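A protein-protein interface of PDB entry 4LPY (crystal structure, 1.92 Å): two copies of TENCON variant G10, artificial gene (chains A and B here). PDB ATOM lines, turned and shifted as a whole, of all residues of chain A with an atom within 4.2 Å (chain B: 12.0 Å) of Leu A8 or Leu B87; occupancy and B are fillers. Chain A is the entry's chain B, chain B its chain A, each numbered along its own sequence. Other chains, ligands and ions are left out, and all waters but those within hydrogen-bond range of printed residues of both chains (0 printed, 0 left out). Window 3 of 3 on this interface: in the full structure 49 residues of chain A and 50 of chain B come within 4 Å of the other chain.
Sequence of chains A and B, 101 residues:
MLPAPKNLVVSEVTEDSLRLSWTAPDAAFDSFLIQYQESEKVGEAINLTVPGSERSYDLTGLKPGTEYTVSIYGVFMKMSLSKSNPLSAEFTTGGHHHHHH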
ATOM      1  N   PRO A   5     -32.776 -19.545 -18.532  1.00  0.00           N
ATOM      2  CA  PRO A   5     -32.329 -20.146 -17.271  1.00  0.00           C
ATOM      3  C   PRO A   5     -31.451 -19.157 -16.514  1.00  0.00           C
ATOM      4  O   PRO A   5     -30.810 -18.298 -17.133  1.00  0.00           O
ATOM      5  CB  PRO A   5     -31.486 -21.344 -17.722  1.00  0.00           C
ATOM      6  CG  PRO A   5     -31.828 -21.577 -19.140  1.00  0.00           C
ATOM      7  CD  PRO A   5     -32.245 -20.252 -19.708  1.00  0.00           C
ATOM      8  N   LYS A   6     -31.416 -19.269 -15.188  1.00  0.00           N
ATOM      9  CA  LYS A   6     -30.560 -18.395 -14.390  1.00  0.00           C
ATOM     10  C   LYS A   6     -29.725 -19.197 -13.394  1.00  0.00           C
ATOM     11  O   LYS A   6     -29.952 -20.399 -13.203  1.00  0.00           O
ATOM     12  CB  LYS A   6     -31.394 -17.349 -13.647  1.00  0.00           C
ATOM     13  CG  LYS A   6     -32.093 -16.341 -14.554  1.00  0.00           C
ATOM     14  CD  LYS A   6     -32.701 -15.202 -13.761  1.00  0.00           C
ATOM     15  CE  LYS A   6     -33.342 -14.184 -14.695  1.00  0.00           C
ATOM     16  NZ  LYS A   6     -33.973 -13.063 -13.950  1.00  0.00           N
ATOM     17  N   ASN A   7     -28.758 -18.525 -12.762  1.00  0.00           N
ATOM     18  CA  ASN A   7     -28.045 -19.107 -11.623  1.00  0.00           C
ATOM     19  C   ASN A   7     -27.389 -20.451 -11.937  1.00  0.00           C
ATOM     20  O   ASN A   7     -27.592 -21.446 -11.248  1.00  0.00           O
ATOM     21  CB  ASN A   7     -28.991 -19.208 -10.419  1.00  0.00           C
ATOM     22  CG  ASN A   7     -29.618 -17.866 -10.077  1.00  0.00           C
ATOM     23  OD1 ASN A   7     -28.922 -16.863 -10.007  1.00  0.00           O
ATOM     24  ND2 ASN A   7     -30.925 -17.845  -9.866  1.00  0.00           N
ATOM     25  N   LEU A   8     -26.590 -20.465 -12.996  1.00  0.00           N
ATOM     26  CA  LEU A   8     -25.842 -21.666 -13.346  1.00  0.00           C
ATOM     27  C   LEU A   8     -24.607 -21.782 -12.455  1.00  0.00           C
ATOM     28  O   LEU A   8     -23.709 -20.944 -12.513  1.00  0.00           O
ATOM     29  CB  LEU A   8     -25.440 -21.644 -14.828  1.00  0.00           C
ATOM     30  CG  LEU A   8     -24.549 -22.794 -15.323  1.00  0.00           C
ATOM     31  CD1 LEU A   8     -25.274 -24.166 -15.327  1.00  0.00           C
ATOM     32  CD2 LEU A   8     -24.014 -22.455 -16.686  1.00  0.00           C
ATOM     33  N   VAL A   9     -24.584 -22.829 -11.637  1.00  0.00           N
ATOM     34  CA  VAL A   9     -23.496 -23.090 -10.692  1.00  0.00           C
ATOM     35  C   VAL A   9     -23.138 -24.584 -10.801  1.00  0.00           C
ATOM     36  O   VAL A   9     -23.834 -25.352 -11.490  1.00  0.00           O
ATOM     37  CB  VAL A   9     -23.904 -22.725  -9.226  1.00  0.00           C
ATOM     38  CG1 VAL A   9     -24.400 -21.266  -9.109  1.00  0.00           C
ATOM     39  CG2 VAL A   9     -24.950 -23.673  -8.675  1.00  0.00           C
ATOM     40  N   SER A  21     -26.085 -27.158 -11.728  1.00  0.00           N
ATOM     41  CA  SER A  21     -27.384 -26.828 -11.154  1.00  0.00           C
ATOM     42  C   SER A  21     -27.794 -25.453 -11.678  1.00  0.00           C
ATOM     43  O   SER A  21     -26.949 -24.592 -11.866  1.00  0.00           O
ATOM     44  CB  SER A  21     -27.310 -26.873  -9.624  1.00  0.00           C
ATOM     45  OG  SER A  21     -28.410 -26.222  -9.046  1.00  0.00           O
ATOM     46  N   VAL A  70     -19.568 -23.907 -20.047  1.00  0.00           N
ATOM     47  CA  VAL A  70     -20.873 -24.591 -20.038  1.00  0.00           C
ATOM     48  C   VAL A  70     -21.946 -23.553 -20.374  1.00  0.00           C
ATOM     49  O   VAL A  70     -21.988 -22.480 -19.772  1.00  0.00           O
ATOM     50  CB  VAL A  70     -21.192 -25.225 -18.649  1.00  0.00           C
ATOM     51  CG1 VAL A  70     -22.582 -25.887 -18.643  1.00  0.00           C
ATOM     52  CG2 VAL A  70     -20.117 -26.264 -18.244  1.00  0.00           C
ATOM     53  N   SER A  71     -22.809 -23.875 -21.336  1.00  0.00           N
ATOM     54  CA  SER A  71     -23.911 -23.001 -21.685  1.00  0.00           C
ATOM     55  C   SER A  71     -25.182 -23.798 -21.540  1.00  0.00           C
ATOM     56  O   SER A  71     -25.235 -24.993 -21.888  1.00  0.00           O
ATOM     57  CB  SER A  71     -23.797 -22.491 -23.127  1.00  0.00           C
ATOM     58  OG  SER A  71     -22.634 -21.716 -23.309  1.00  0.00           O
ATOM     59  N   ILE A  72     -26.208 -23.136 -21.026  1.00  0.00           N
ATOM     60  CA  ILE A  72     -27.525 -23.732 -20.978  1.00  0.00           C
ATOM     61  C   ILE A  72     -28.541 -22.822 -21.667  1.00  0.00           C
ATOM     62  O   ILE A  72     -28.561 -21.606 -21.439  1.00  0.00           O
ATOM     63  CB  ILE A  72     -27.941 -24.129 -19.540  1.00  0.00           C
ATOM     64  CG1 ILE A  72     -29.319 -24.795 -19.553  1.00  0.00           C
ATOM     65  CG2 ILE A  72     -27.898 -22.902 -18.581  1.00  0.00           C
ATOM     66  CD1 ILE A  72     -29.611 -25.634 -18.356  1.00  0.00           C
ATOM     67  N   LYS B  83     -35.457 -21.286 -28.725  1.00  0.00           N
ATOM     68  CA  LYS B  83     -34.368 -21.394 -27.784  1.00  0.00           C
ATOM     69  C   LYS B  83     -34.240 -20.032 -27.122  1.00  0.00           C
ATOM     70  O   LYS B  83     -34.272 -19.014 -27.814  1.00  0.00           O
ATOM     71  CB  LYS B  83     -33.106 -21.629 -28.594  1.00  0.00           C
ATOM     72  CG  LYS B  83     -32.284 -22.811 -28.244  1.00  0.00           C
ATOM     73  CD  LYS B  83     -31.316 -23.023 -29.393  1.00  0.00           C
ATOM     74  CE  LYS B  83     -29.957 -23.456 -28.919  1.00  0.00           C
ATOM     75  NZ  LYS B  83     -28.934 -23.342 -29.997  1.00  0.00           N
ATOM     76  N   SER B  84     -34.096 -20.002 -25.799  1.00  0.00           N
ATOM     77  CA  SER B  84     -33.753 -18.770 -25.081  1.00  0.00           C
ATOM     78  C   SER B  84     -32.314 -18.366 -25.401  1.00  0.00           C
ATOM     79  O   SER B  84     -31.558 -19.145 -26.008  1.00  0.00           O
ATOM     80  CB  SER B  84     -33.866 -18.987 -23.563  1.00  0.00           C
ATOM     81  OG  SER B  84     -32.689 -19.622 -23.054  1.00  0.00           O
ATOM     82  N   ASN B  85     -31.935 -17.153 -24.993  1.00  0.00           N
ATOM     83  CA  ASN B  85     -30.522 -16.780 -24.909  1.00  0.00           C
ATOM     84  C   ASN B  85     -29.827 -17.735 -23.937  1.00  0.00           C
ATOM     85  O   ASN B  85     -30.431 -18.129 -22.933  1.00  0.00           O
ATOM     86  CB  ASN B  85     -30.358 -15.340 -24.400  1.00  0.00           C
ATOM     87  CG  ASN B  85     -30.959 -14.306 -25.345  1.00  0.00           C
ATOM     88  OD1 ASN B  85     -30.651 -14.280 -26.538  1.00  0.00           O
ATOM     89  ND2 ASN B  85     -31.820 -13.451 -24.810  1.00  0.00           N
ATOM     90  N   PRO B  86     -28.567 -18.109 -24.226  1.00  0.00           N
ATOM     91  CA  PRO B  86     -27.902 -19.040 -23.316  1.00  0.00           C
ATOM     92  C   PRO B  86     -27.528 -18.381 -21.992  1.00  0.00           C
ATOM     93  O   PRO B  86     -27.393 -17.162 -21.909  1.00  0.00           O
ATOM     94  CB  PRO B  86     -26.638 -19.441 -24.080  1.00  0.00           C
ATOM     95  CG  PRO B  86     -26.356 -18.280 -24.979  1.00  0.00           C
ATOM     96  CD  PRO B  86     -27.700 -17.721 -25.360  1.00  0.00           C
ATOM     97  N   LEU B  87     -27.363 -19.195 -20.961  1.00  0.00           N
ATOM     98  CA  LEU B  87     -26.637 -18.754 -19.786  1.00  0.00           C
ATOM     99  C   LEU B  87     -25.344 -19.556 -19.735  1.00  0.00           C
ATOM    100  O   LEU B  87     -25.370 -20.772 -19.814  1.00  0.00           O
ATOM    101  CB  LEU B  87     -27.456 -18.962 -18.513  1.00  0.00           C
ATOM    102  CG  LEU B  87     -26.732 -18.649 -17.198  1.00  0.00           C
ATOM    103  CD1 LEU B  87     -26.339 -17.169 -17.061  1.00  0.00           C
ATOM    104  CD2 LEU B  87     -27.590 -19.071 -16.057  1.00  0.00           C
ATOM    105  N   SER B  88     -24.222 -18.861 -19.603  1.00  0.00           N
ATOM    106  CA  SER B  88     -22.921 -19.492 -19.687  1.00  0.00           C
ATOM    107  C   SER B  88     -22.098 -19.192 -18.438  1.00  0.00           C
ATOM    108  O   SER B  88     -22.252 -18.126 -17.822  1.00  0.00           O
ATOM    109  CB  SER B  88     -22.188 -19.018 -20.943  1.00  0.00           C
ATOM    110  OG  SER B  88     -22.907 -19.374 -22.112  1.00  0.00           O
ATOM    111  N   ALA B  89     -21.234 -20.138 -18.082  1.00  0.00           N
ATOM    112  CA  ALA B  89     -20.286 -19.995 -16.962  1.00  0.00           C
ATOM    113  C   ALA B  89     -19.082 -20.886 -17.235  1.00  0.00           C
ATOM    114  O   ALA B  89     -19.162 -21.834 -18.037  1.00  0.00           O
ATOM    115  CB  ALA B  89     -20.947 -20.369 -15.624  1.00  0.00           C
ATOM    116  N   GLU B  90     -17.966 -20.582 -16.570  1.00  0.00           N
ATOM    117  CA  GLU B  90     -16.782 -21.428 -16.629  1.00  0.00           C
ATOM    118  C   GLU B  90     -16.575 -22.099 -15.282  1.00  0.00           C
ATOM    119  O   GLU B  90     -16.764 -21.475 -14.227  1.00  0.00           O
ATOM    120  CB  GLU B  90     -15.543 -20.616 -17.044  1.00  0.00           C
ATOM    121  CG  GLU B  90     -15.636 -20.100 -18.489  1.00  0.00           C
ATOM    122  CD  GLU B  90     -14.771 -18.884 -18.763  1.00  0.00           C
ATOM    123  OE1 GLU B  90     -14.141 -18.355 -17.821  1.00  0.00           O
ATOM    124  OE2 GLU B  90     -14.726 -18.458 -19.935  1.00  0.00           O
ATOM    125  N   PHE B  91     -16.187 -23.372 -15.321  1.00  0.00           N
ATOM    126  CA  PHE B  91     -15.951 -24.137 -14.099  1.00  0.00           C
ATOM    127  C   PHE B  91     -14.667 -24.902 -14.251  1.00  0.00           C
ATOM    128  O   PHE B  91     -14.291 -25.253 -15.370  1.00  0.00           O
ATOM    129  CB  PHE B  91     -17.098 -25.133 -13.830  1.00  0.00           C
ATOM    130  CG  PHE B  91     -18.446 -24.490 -13.711  1.00  0.00           C
ATOM    131  CD1 PHE B  91     -18.783 -23.757 -12.577  1.00  0.00           C
ATOM    132  CD2 PHE B  91     -19.385 -24.617 -14.736  1.00  0.00           C
ATOM    133  CE1 PHE B  91     -20.042 -23.154 -12.461  1.00  0.00           C
ATOM    134  CE2 PHE B  91     -20.652 -24.017 -14.634  1.00  0.00           C
ATOM    135  CZ  PHE B  91     -20.982 -23.286 -13.497  1.00  0.00           C
ATOM    136  N   THR B  92     -13.998 -25.160 -13.130  1.00  0.00           N
ATOM    137  CA  THR B  92     -12.766 -25.940 -13.152  1.00  0.00           C
ATOM    138  C   THR B  92     -12.937 -27.235 -12.386  1.00  0.00           C
ATOM    139  O   THR B  92     -13.389 -27.239 -11.236  1.00  0.00           O
ATOM    140  CB  THR B  92     -11.571 -25.128 -12.596  1.00  0.00           C
ATOM    141  OG1 THR B  92     -11.409 -23.939 -13.381  1.00  0.00           O
ATOM    142  CG2 THR B  92     -10.285 -25.940 -12.638  1.00  0.00           C
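No position is printed for both chains.
O of Ile A72 is in hydrogen-bond range of N of Leu B87.
The side-chain hydroxyl (OG) of Ser B88 sits at hydrogen-bond distance from the side-chain hydroxyl (OG) of Ser A71, at 2.6 Å.
The backbone NH (N) of Val A70 lies within hydrogen-bond range of the backbone carbonyl oxygen (O) of Ala B89.
Printed residues of chain B within 4 Å of Asn A7: Leu B87.
Of chain B, only Phe B91 (3.7 Å) comes within 4 Å of Val A9.
Of the printed residues of chain A, Pro B86 touches Ile A72 (3.2 Å).
Of chain A, only Pro A5, Lys A6, Asn A7, Leu A8, Val A70, Ser A71 and Ile A72 come within 4 Å of Leu B87.
Of the printed residues of chain A, Ala B89 touches Leu A8 and Val A70.
The nearest printed residue of chain A that does not touch Leu B87 is Val A9 (6.5 Å).
The nearest printed residue of chain A that does not touch Ser B84 is Ile A72 (4.9 Å).
The backbone carbonyl oxygen (O) of Val A9 is in hydrogen-bond range of the backbone NH (N) of Ser A21 (2.9 Å).
Of the 9 printed residues of chain A, 8 touch a printed residue of chain B.
Hydrophobic or aromatic side chains of chain A within 4 Å of the printed part of chain B: Pro A5, Leu A8, Val A70 and Ile A72.
Among the printed residues, no Asp or Glu carboxylate lies within 4 Å of a Lys or Arg side-chain nitrogen of the other chain.
CD of Pro A5 touches OG of Ser B84, at 3.4 Å.
O of Pro A5 touches CD2 of Leu B87 (3.5 Å).
Lys A6 touches Leu B87 (C to CD2, 3.4 Å).
CD2 of Leu B87 touches N of Leu A8 (3.5 Å).
CD2 of Leu A8 touches CB of Ala B89 (3.9 Å).
Leu A8 touches Phe B91.
Val A9 touches Phe B91.
O of Val A70 touches O of Leu B87, 3.8 Å away.
Ser A71 touches Leu B87.
Ile A72 touches Pro B86.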
